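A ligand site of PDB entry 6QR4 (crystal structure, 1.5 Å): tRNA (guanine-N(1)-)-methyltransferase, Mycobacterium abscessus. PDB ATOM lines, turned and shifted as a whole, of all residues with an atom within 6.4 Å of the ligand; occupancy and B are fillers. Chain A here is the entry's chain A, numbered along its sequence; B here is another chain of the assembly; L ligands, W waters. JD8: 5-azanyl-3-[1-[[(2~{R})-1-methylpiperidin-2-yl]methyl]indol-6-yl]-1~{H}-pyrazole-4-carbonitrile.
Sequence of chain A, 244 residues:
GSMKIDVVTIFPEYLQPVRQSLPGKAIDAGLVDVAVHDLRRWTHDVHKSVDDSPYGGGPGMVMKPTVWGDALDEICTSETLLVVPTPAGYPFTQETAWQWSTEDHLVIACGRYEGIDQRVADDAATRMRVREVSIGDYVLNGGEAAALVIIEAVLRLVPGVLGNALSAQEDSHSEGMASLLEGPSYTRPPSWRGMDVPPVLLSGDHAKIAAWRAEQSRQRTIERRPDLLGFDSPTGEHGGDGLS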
ATOM      1  N   VAL A  84      15.998   4.095  23.758  1.00  0.00           N
ATOM      2  CA  VAL A  84      16.343   5.500  23.945  1.00  0.00           C
ATOM      3  C   VAL A  84      17.581   5.623  24.815  1.00  0.00           C
ATOM      4  O   VAL A  84      17.507   5.488  26.038  1.00  0.00           O
ATOM      5  CB  VAL A  84      15.191   6.267  24.609  1.00  0.00           C
ATOM      6  CG1 VAL A  84      15.528   7.760  24.680  1.00  0.00           C
ATOM      7  CG2 VAL A  84      13.870   6.015  23.878  1.00  0.00           C
ATOM      8  N   PRO A  85      18.741   5.839  24.186  1.00  0.00           N
ATOM      9  CA  PRO A  85      19.927   6.065  25.010  1.00  0.00           C
ATOM     10  C   PRO A  85      19.767   7.308  25.876  1.00  0.00           C
ATOM     11  O   PRO A  85      19.199   8.316  25.452  1.00  0.00           O
ATOM     12  CB  PRO A  85      21.056   6.240  23.990  1.00  0.00           C
ATOM     13  CG  PRO A  85      20.550   5.498  22.739  1.00  0.00           C
ATOM     14  CD  PRO A  85      19.055   5.773  22.750  1.00  0.00           C
ATOM     15  N   THR A  86      20.257   7.217  27.103  1.00  0.00           N
ATOM     16  CA  THR A  86      20.220   8.332  28.041  1.00  0.00           C
ATOM     17  C   THR A  86      21.157   8.009  29.194  1.00  0.00           C
ATOM     18  O   THR A  86      21.234   6.867  29.618  1.00  0.00           O
ATOM     19  CB  THR A  86      18.784   8.617  28.571  1.00  0.00           C
ATOM     20  OG1 THR A  86      18.878   9.398  29.768  1.00  0.00           O
ATOM     21  CG2 THR A  86      17.985   7.329  28.822  1.00  0.00           C
ATOM     22  N   PRO A  87      21.875   9.027  29.686  1.00  0.00           N
ATOM     23  CA  PRO A  87      22.752   8.768  30.843  1.00  0.00           C
ATOM     24  C   PRO A  87      21.947   8.393  32.078  1.00  0.00           C
ATOM     25  O   PRO A  87      22.537   7.864  33.019  1.00  0.00           O
ATOM     26  CB  PRO A  87      23.488  10.109  31.027  1.00  0.00           C
ATOM     27  CG  PRO A  87      22.592  11.116  30.411  1.00  0.00           C
ATOM     28  CD  PRO A  87      21.867  10.431  29.283  1.00  0.00           C
ATOM     29  N   ALA A  88      20.636   8.634  32.070  1.00  0.00           N
ATOM     30  CA  ALA A  88      19.757   8.286  33.174  1.00  0.00           C
ATOM     31  C   ALA A  88      19.057   6.932  32.956  1.00  0.00           C
ATOM     32  O   ALA A  88      18.099   6.602  33.660  1.00  0.00           O
ATOM     33  CB  ALA A  88      18.716   9.386  33.385  1.00  0.00           C
ATOM     34  N   CYS A 110      18.008   8.738  19.012  1.00  0.00           N
ATOM     35  CA  CYS A 110      19.200   9.397  19.503  1.00  0.00           C
ATOM     36  C   CYS A 110      18.933  10.838  19.859  1.00  0.00           C
ATOM     37  O   CYS A 110      18.677  11.641  18.971  1.00  0.00           O
ATOM     38  CB  CYS A 110      20.319   9.353  18.466  1.00  0.00           C
ATOM     39  SG  CYS A 110      20.889   7.698  18.043  1.00  0.00           S
ATOM     40  N   GLY A 111      19.034  11.182  21.133  1.00  0.00           N
ATOM     41  CA  GLY A 111      18.892  12.579  21.530  1.00  0.00           C
ATOM     42  C   GLY A 111      20.197  13.369  21.452  1.00  0.00           C
ATOM     43  O   GLY A 111      21.281  12.805  21.313  1.00  0.00           O
ATOM     44  N   ARG A 112      20.046  14.674  21.546  1.00  0.00           N
ATOM     45  CA  ARG A 112      21.140  15.623  21.710  1.00  0.00           C
ATOM     46  C   ARG A 112      20.708  16.655  22.744  1.00  0.00           C
ATOM     47  O   ARG A 112      19.555  16.627  23.207  1.00  0.00           O
ATOM     48  CB  ARG A 112      21.502  16.282  20.372  1.00  0.00           C
ATOM     49  CG  ARG A 112      22.330  15.407  19.440  1.00  0.00           C
ATOM     50  CD  ARG A 112      23.821  15.643  19.669  1.00  0.00           C
ATOM     51  NE  ARG A 112      24.608  14.463  19.326  1.00  0.00           N
ATOM     52  CZ  ARG A 112      25.926  14.442  19.246  1.00  0.00           C
ATOM     53  NH1 ARG A 112      26.614  15.567  19.460  1.00  0.00           N
ATOM     54  NH2 ARG A 112      26.568  13.325  18.939  1.00  0.00           N
ATOM     55  N   TYR A 113      21.623  17.572  23.091  1.00  0.00           N
ATOM     56  CA  TYR A 113      21.333  18.670  24.010  1.00  0.00           C
ATOM     57  C   TYR A 113      20.946  18.094  25.367  1.00  0.00           C
ATOM     58  O   TYR A 113      21.654  17.195  25.852  1.00  0.00           O
ATOM     59  CB  TYR A 113      20.266  19.579  23.416  1.00  0.00           C
ATOM     60  CG  TYR A 113      20.587  19.871  21.976  1.00  0.00           C
ATOM     61  CD1 TYR A 113      21.885  20.239  21.613  1.00  0.00           C
ATOM     62  CD2 TYR A 113      19.642  19.708  20.978  1.00  0.00           C
ATOM     63  CE1 TYR A 113      22.223  20.472  20.301  1.00  0.00           C
ATOM     64  CE2 TYR A 113      19.965  19.957  19.644  1.00  0.00           C
ATOM     65  CZ  TYR A 113      21.264  20.335  19.324  1.00  0.00           C
ATOM     66  OH  TYR A 113      21.619  20.573  18.013  1.00  0.00           O
ATOM     67  N   GLU A 114      19.882  18.554  25.998  1.00  0.00           N
ATOM     68  CA  GLU A 114      19.550  18.001  27.314  1.00  0.00           C
ATOM     69  C   GLU A 114      18.855  16.656  27.203  1.00  0.00           C
ATOM     70  O   GLU A 114      18.732  15.924  28.192  1.00  0.00           O
ATOM     71  CB  GLU A 114      18.676  18.978  28.116  1.00  0.00           C
ATOM     72  CG  GLU A 114      19.379  20.288  28.426  1.00  0.00           C
ATOM     73  CD  GLU A 114      20.691  20.076  29.184  1.00  0.00           C
ATOM     74  OE1 GLU A 114      21.759  20.399  28.613  1.00  0.00           O
ATOM     75  OE2 GLU A 114      20.651  19.601  30.329  1.00  0.00           O
ATOM     76  N   GLY A 115      18.424  16.302  25.991  1.00  0.00           N
ATOM     77  CA  GLY A 115      17.708  15.070  25.743  1.00  0.00           C
ATOM     78  C   GLY A 115      16.360  15.347  25.102  1.00  0.00           C
ATOM     79  O   GLY A 115      16.098  16.448  24.635  1.00  0.00           O
ATOM     80  N   ILE A 116      15.519  14.329  25.092  1.00  0.00           N
ATOM     81  CA  ILE A 116      14.222  14.408  24.429  1.00  0.00           C
ATOM     82  C   ILE A 116      13.120  14.669  25.450  1.00  0.00           C
ATOM     83  O   ILE A 116      13.137  14.067  26.521  1.00  0.00           O
ATOM     84  CB  ILE A 116      13.938  13.109  23.656  1.00  0.00           C
ATOM     85  CG1 ILE A 116      15.097  12.785  22.703  1.00  0.00           C
ATOM     86  CG2 ILE A 116      12.586  13.154  22.934  1.00  0.00           C
ATOM     87  CD1 ILE A 116      14.960  11.435  22.044  1.00  0.00           C
ATOM     88  N   VAL A 133      18.102   3.332  28.222  1.00  0.00           N
ATOM     89  CA  VAL A 133      19.312   2.659  28.684  1.00  0.00           C
ATOM     90  C   VAL A 133      20.549   3.526  28.566  1.00  0.00           C
ATOM     91  O   VAL A 133      20.604   4.431  27.741  1.00  0.00           O
ATOM     92  CB  VAL A 133      19.598   1.339  27.917  1.00  0.00           C
ATOM     93  CG1 VAL A 133      18.478   0.346  28.113  1.00  0.00           C
ATOM     94  CG2 VAL A 133      19.828   1.600  26.423  1.00  0.00           C
ATOM     95  N   SER A 134      21.544   3.215  29.403  1.00  0.00           N
ATOM     96  CA  SER A 134      22.831   3.873  29.354  1.00  0.00           C
ATOM     97  C   SER A 134      23.944   2.865  29.110  1.00  0.00           C
ATOM     98  O   SER A 134      23.953   1.789  29.706  1.00  0.00           O
ATOM     99  CB  SER A 134      23.100   4.593  30.680  1.00  0.00           C
ATOM    100  OG  SER A 134      24.451   5.037  30.701  1.00  0.00           O
ATOM    101  N   ILE A 135      24.895   3.219  28.242  1.00  0.00           N
ATOM    102  CA  ILE A 135      26.010   2.294  27.954  1.00  0.00           C
ATOM    103  C   ILE A 135      27.178   2.409  28.948  1.00  0.00           C
ATOM    104  O   ILE A 135      28.112   1.623  28.883  1.00  0.00           O
ATOM    105  CB  ILE A 135      26.558   2.485  26.504  1.00  0.00           C
ATOM    106  CG1 ILE A 135      27.046   3.914  26.265  1.00  0.00           C
ATOM    107  CG2 ILE A 135      25.490   2.101  25.504  1.00  0.00           C
ATOM    108  CD1 ILE A 135      28.126   4.000  25.153  1.00  0.00           C
ATOM    109  N   GLY A 136      27.107   3.345  29.901  1.00  0.00           N
ATOM    110  CA  GLY A 136      28.173   3.444  30.884  1.00  0.00           C
ATOM    111  C   GLY A 136      28.159   4.731  31.678  1.00  0.00           C
ATOM    112  O   GLY A 136      27.413   5.653  31.354  1.00  0.00           O
ATOM    113  N   ASP A 137      28.998   4.793  32.722  1.00  0.00           N
ATOM    114  CA  ASP A 137      28.964   5.917  33.659  1.00  0.00           C
ATOM    115  C   ASP A 137      29.931   7.018  33.263  1.00  0.00           C
ATOM    116  O   ASP A 137      30.913   7.306  33.956  1.00  0.00           O
ATOM    117  CB  ASP A 137      29.256   5.419  35.068  1.00  0.00           C
ATOM    118  CG  ASP A 137      28.080   4.667  35.668  1.00  0.00           C
ATOM    119  OD1 ASP A 137      26.944   4.869  35.188  1.00  0.00           O
ATOM    120  OD2 ASP A 137      28.282   3.894  36.624  1.00  0.00           O
ATOM    121  N   TYR A 138      29.623   7.638  32.135  1.00  0.00           N
ATOM    122  CA  TYR A 138      30.352   8.771  31.600  1.00  0.00           C
ATOM    123  C   TYR A 138      29.331   9.547  30.805  1.00  0.00           C
ATOM    124  O   TYR A 138      28.245   9.020  30.493  1.00  0.00           O
ATOM    125  CB  TYR A 138      31.535   8.333  30.713  1.00  0.00           C
ATOM    126  CG  TYR A 138      31.235   7.093  29.918  1.00  0.00           C
ATOM    127  CD1 TYR A 138      30.427   7.147  28.775  1.00  0.00           C
ATOM    128  CD2 TYR A 138      31.706   5.854  30.326  1.00  0.00           C
ATOM    129  CE1 TYR A 138      30.129   6.013  28.077  1.00  0.00           C
ATOM    130  CE2 TYR A 138      31.412   4.707  29.621  1.00  0.00           C
ATOM    131  CZ  TYR A 138      30.623   4.798  28.500  1.00  0.00           C
ATOM    132  OH  TYR A 138      30.315   3.656  27.795  1.00  0.00           O
ATOM    133  N   VAL A 139      29.666  10.787  30.491  1.00  0.00           N
ATOM    134  CA  VAL A 139      28.743  11.688  29.825  1.00  0.00           C
ATOM    135  C   VAL A 139      29.181  11.885  28.377  1.00  0.00           C
ATOM    136  O   VAL A 139      30.342  12.196  28.101  1.00  0.00           O
ATOM    137  CB  VAL A 139      28.670  13.049  30.545  1.00  0.00           C
ATOM    138  CG1 VAL A 139      27.698  13.978  29.835  1.00  0.00           C
ATOM    139  CG2 VAL A 139      28.271  12.859  32.002  1.00  0.00           C
ATOM    140  N   LEU A 140      28.246  11.677  27.452  1.00  0.00           N
ATOM    141  CA  LEU A 140      28.463  11.931  26.035  1.00  0.00           C
ATOM    142  C   LEU A 140      27.686  13.172  25.591  1.00  0.00           C
ATOM    143  O   LEU A 140      26.909  13.722  26.368  1.00  0.00           O
ATOM    144  CB  LEU A 140      28.014  10.712  25.211  1.00  0.00           C
ATOM    145  CG  LEU A 140      28.665   9.389  25.629  1.00  0.00           C
ATOM    146  CD1 LEU A 140      27.899   8.218  25.009  1.00  0.00           C
ATOM    147  CD2 LEU A 140      30.142   9.344  25.232  1.00  0.00           C
ATOM    148  N   ASN A 141      27.884  13.592  24.348  1.00  0.00           N
ATOM    149  CA  ASN A 141      27.146  14.735  23.787  1.00  0.00           C
ATOM    150  C   ASN A 141      25.750  14.370  23.303  1.00  0.00           C
ATOM    151  O   ASN A 141      24.909  15.252  23.088  1.00  0.00           O
ATOM    152  CB  ASN A 141      27.914  15.356  22.632  1.00  0.00           C
ATOM    153  CG  ASN A 141      29.218  15.986  23.072  1.00  0.00           C
ATOM    154  OD1 ASN A 141      29.277  16.643  24.113  1.00  0.00           O
ATOM    155  ND2 ASN A 141      30.266  15.776  22.289  1.00  0.00           N
ATOM    156  N   GLY A 142      25.500  13.080  23.084  1.00  0.00           N
ATOM    157  CA  GLY A 142      24.203  12.671  22.569  1.00  0.00           C
ATOM    158  C   GLY A 142      24.162  11.158  22.441  1.00  0.00           C
ATOM    159  O   GLY A 142      25.100  10.475  22.849  1.00  0.00           O
ATOM    160  N   GLY A 143      23.085  10.638  21.854  1.00  0.00           N
ATOM    161  CA  GLY A 143      22.879   9.205  21.823  1.00  0.00           C
ATOM    162  C   GLY A 143      23.597   8.422  20.728  1.00  0.00           C
ATOM    163  O   GLY A 143      23.589   7.194  20.767  1.00  0.00           O
ATOM    164  N   GLU A 144      24.212   9.107  19.777  1.00  0.00           N
ATOM    165  CA  GLU A 144      24.761   8.427  18.602  1.00  0.00           C
ATOM    166  C   GLU A 144      25.870   7.429  18.930  1.00  0.00           C
ATOM    167  O   GLU A 144      25.863   6.298  18.430  1.00  0.00           O
ATOM    168  CB  GLU A 144      25.285   9.463  17.591  1.00  0.00           C
ATOM    169  CG  GLU A 144      24.174  10.229  16.884  1.00  0.00           C
ATOM    170  CD  GLU A 144      23.578  11.362  17.710  1.00  0.00           C
ATOM    171  OE1 GLU A 144      24.101  11.684  18.806  1.00  0.00           O
ATOM    172  OE2 GLU A 144      22.582  11.938  17.237  1.00  0.00           O
ATOM    173  N   ALA A 146      26.292   5.928  21.690  1.00  0.00           N
ATOM    174  CA  ALA A 146      25.612   4.852  22.390  1.00  0.00           C
ATOM    175  C   ALA A 146      24.914   3.924  21.394  1.00  0.00           C
ATOM    176  O   ALA A 146      24.956   2.710  21.570  1.00  0.00           O
ATOM    177  CB  ALA A 146      24.600   5.410  23.410  1.00  0.00           C
ATOM    178  N   ILE A 150      25.454  -0.096  21.047  1.00  0.00           N
ATOM    179  CA  ILE A 150      24.314  -1.008  21.163  1.00  0.00           C
ATOM    180  C   ILE A 150      24.133  -1.833  19.893  1.00  0.00           C
ATOM    181  O   ILE A 150      23.922  -3.053  19.986  1.00  0.00           O
ATOM    182  CB  ILE A 150      23.021  -0.222  21.481  1.00  0.00           C
ATOM    183  CG1 ILE A 150      23.098   0.331  22.906  1.00  0.00           C
ATOM    184  CG2 ILE A 150      21.778  -1.108  21.301  1.00  0.00           C
ATOM    185  CD1 ILE A 150      22.115   1.475  23.176  1.00  0.00           C
ATOM    186  N   ARG B 156      35.003  16.597  25.322  1.00  0.00           N
ATOM    187  CA  ARG B 156      34.046  17.604  25.744  1.00  0.00           C
ATOM    188  C   ARG B 156      34.440  18.236  27.098  1.00  0.00           C
ATOM    189  O   ARG B 156      33.856  19.238  27.524  1.00  0.00           O
ATOM    190  CB  ARG B 156      32.641  16.998  25.815  1.00  0.00           C
ATOM    191  CG  ARG B 156      32.503  15.857  26.774  1.00  0.00           C
ATOM    192  CD  ARG B 156      31.114  15.203  26.641  1.00  0.00           C
ATOM    193  NE  ARG B 156      30.038  16.135  26.967  1.00  0.00           N
ATOM    194  CZ  ARG B 156      29.713  16.481  28.214  1.00  0.00           C
ATOM    195  NH1 ARG B 156      30.399  16.004  29.251  1.00  0.00           N
ATOM    196  NH2 ARG B 156      28.718  17.332  28.445  1.00  0.00           N
ATOM    197  N   GLU B 182      20.012  12.095  36.018  1.00  0.00           N
ATOM    198  CA  GLU B 182      19.233  13.209  35.469  1.00  0.00           C
ATOM    199  C   GLU B 182      17.755  12.873  35.483  1.00  0.00           C
ATOM    200  O   GLU B 182      17.361  11.761  35.184  1.00  0.00           O
ATOM    201  CB  GLU B 182      19.674  13.522  34.041  1.00  0.00           C
ATOM    202  CG  GLU B 182      21.108  14.012  33.909  1.00  0.00           C
ATOM    203  CD  GLU B 182      21.234  15.505  34.148  1.00  0.00           C
ATOM    204  OE1 GLU B 182      20.195  16.181  34.323  1.00  0.00           O
ATOM    205  OE2 GLU B 182      22.382  16.011  34.144  1.00  0.00           O
HETATM  206  C10 JD8 L   1      21.738  10.367  25.122  1.00  0.00           C
HETATM  207  C13 JD8 L   1      21.772  14.100  25.040  1.00  0.00           C
HETATM  208  C15 JD8 L   1      23.823  14.708  26.281  1.00  0.00           C
HETATM  209  C17 JD8 L   1      23.315  14.311  28.727  1.00  0.00           C
HETATM  210  C20 JD8 L   1      23.649  17.099  29.168  1.00  0.00           C
HETATM  211  C22 JD8 L   1      25.308  16.291  27.990  1.00  0.00           C
HETATM  212  C24 JD8 L   1      23.983   6.875  26.921  1.00  0.00           C
HETATM  213  N01 JD8 L   1      26.349   6.586  28.848  1.00  0.00           N
HETATM  214  C02 JD8 L   1      25.891   7.820  28.291  1.00  0.00           C
HETATM  215  N03 JD8 L   1      26.460   9.040  28.555  1.00  0.00           N
HETATM  216  N04 JD8 L   1      25.784   9.980  27.879  1.00  0.00           N
HETATM  217  C05 JD8 L   1      24.816   9.369  27.156  1.00  0.00           C
HETATM  218  C06 JD8 L   1      23.792  10.200  26.367  1.00  0.00           C
HETATM  219  C07 JD8 L   1      23.932  11.604  26.445  1.00  0.00           C
HETATM  220  C08 JD8 L   1      22.951  12.387  25.807  1.00  0.00           C
HETATM  221  C09 JD8 L   1      21.883  11.801  25.164  1.00  0.00           C
HETATM  222  C11 JD8 L   1      22.683   9.586  25.737  1.00  0.00           C
HETATM  223  C12 JD8 L   1      21.118  12.878  24.674  1.00  0.00           C
HETATM  224  N14 JD8 L   1      22.852  13.791  25.711  1.00  0.00           N
HETATM  225  C16 JD8 L   1      23.331  15.336  27.594  1.00  0.00           C
HETATM  226  C18 JD8 L   1      22.768  14.853  29.939  1.00  0.00           C
HETATM  227  C19 JD8 L   1      23.335  16.126  30.315  1.00  0.00           C
HETATM  228  N21 JD8 L   1      24.083  16.512  27.930  1.00  0.00           N
HETATM  229  C23 JD8 L   1      24.817   8.011  27.431  1.00  0.00           C
HETATM  230  N25 JD8 L   1      23.398   5.979  26.581  1.00  0.00           N
HETATM  231  O   HOH W   1      24.581  18.779  25.980  1.00  0.00           O
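O of Tyr 138 sits at hydrogen-bond distance from N03 of the ligand (2.6 Å). The backbone carbonyl oxygen (O) of Tyr 113 lies close to a nitrogen (N21) of the ligand, 3.3 Å away. A nitrogen (N01) of the ligand lies within hydrogen-bond range of the backbone carbonyl oxygen (O) of Gly 136. OG of Ser 134 sits at hydrogen-bond distance from N01 of the ligand (3.1 Å). The backbone NH (N) of Thr 86 lies within hydrogen-bond range of a nitrogen (N25) of the ligand, 3.4 Å away. The backbone NH (N) of Leu 140 sits at hydrogen-bond distance from a nitrogen (N04) of the ligand (3.0 Å).
O of Val 133 lies close to N25 of the ligand, 3.4 Å away. Pro 85 touches the ligand (O to C10, 3.3 Å). Pro 87 touches the ligand (CD to C06, 3.5 Å). O of Gly 111 touches C12 of the ligand (3.4 Å). C of Arg 112 touches C13 of the ligand, at 3.6 Å. Glu 114 touches the ligand. Ile 135 touches the ligand (N to N25, 3.6 Å). Val 139 touches the ligand. Asn 141 touches the ligand. Gly 142 touches the ligand (CA to C08, 3.5 Å). Gly 143 touches the ligand (N to C10, 3.5 Å). Ala 146 touches the ligand (CB to N25, 3.4 Å). NH2 of Arg 156 of chain B touches C22 of the ligand, 3.6 Å away. OE2 of Glu 182 of chain B touches C19 of the ligand, 3.9 Å away. Hydrophobic or aromatic side chains within 4 Å of the ligand: Pro 85, Pro 87, Ile 135, Tyr 138, Val 139, Leu 140 and Ala 146. Of the 28 residues printed, 20 come within 4 Å of the ligand.
OG of Ser 134 lies within hydrogen-bond range of O of Gly 136, 3.1 Å away. OH of Tyr 138 sits at hydrogen-bond distance from O of Ile 135 (3.2 Å). The backbone NH (N) of Val 133 lies within hydrogen-bond range of the backbone carbonyl oxygen (O) of Val 84. The backbone carbonyl oxygen (O) of Gly 111 is in hydrogen-bond range of the backbone NH (N) of Gly 143 (2.9 Å). The backbone carbonyl oxygen (O) of Val 133 lies within hydrogen-bond range of the backbone NH (N) of Thr 86. OD1 of Asn 141 sits at hydrogen-bond distance from NE of Arg 156 of chain B (3.0 Å). OG1 of Thr 86 sits close to N of Ala 88, 3.0 Å away. NE of Arg 112 lies within salt-bridge range of OE1 of Glu 144 (2.9 Å).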
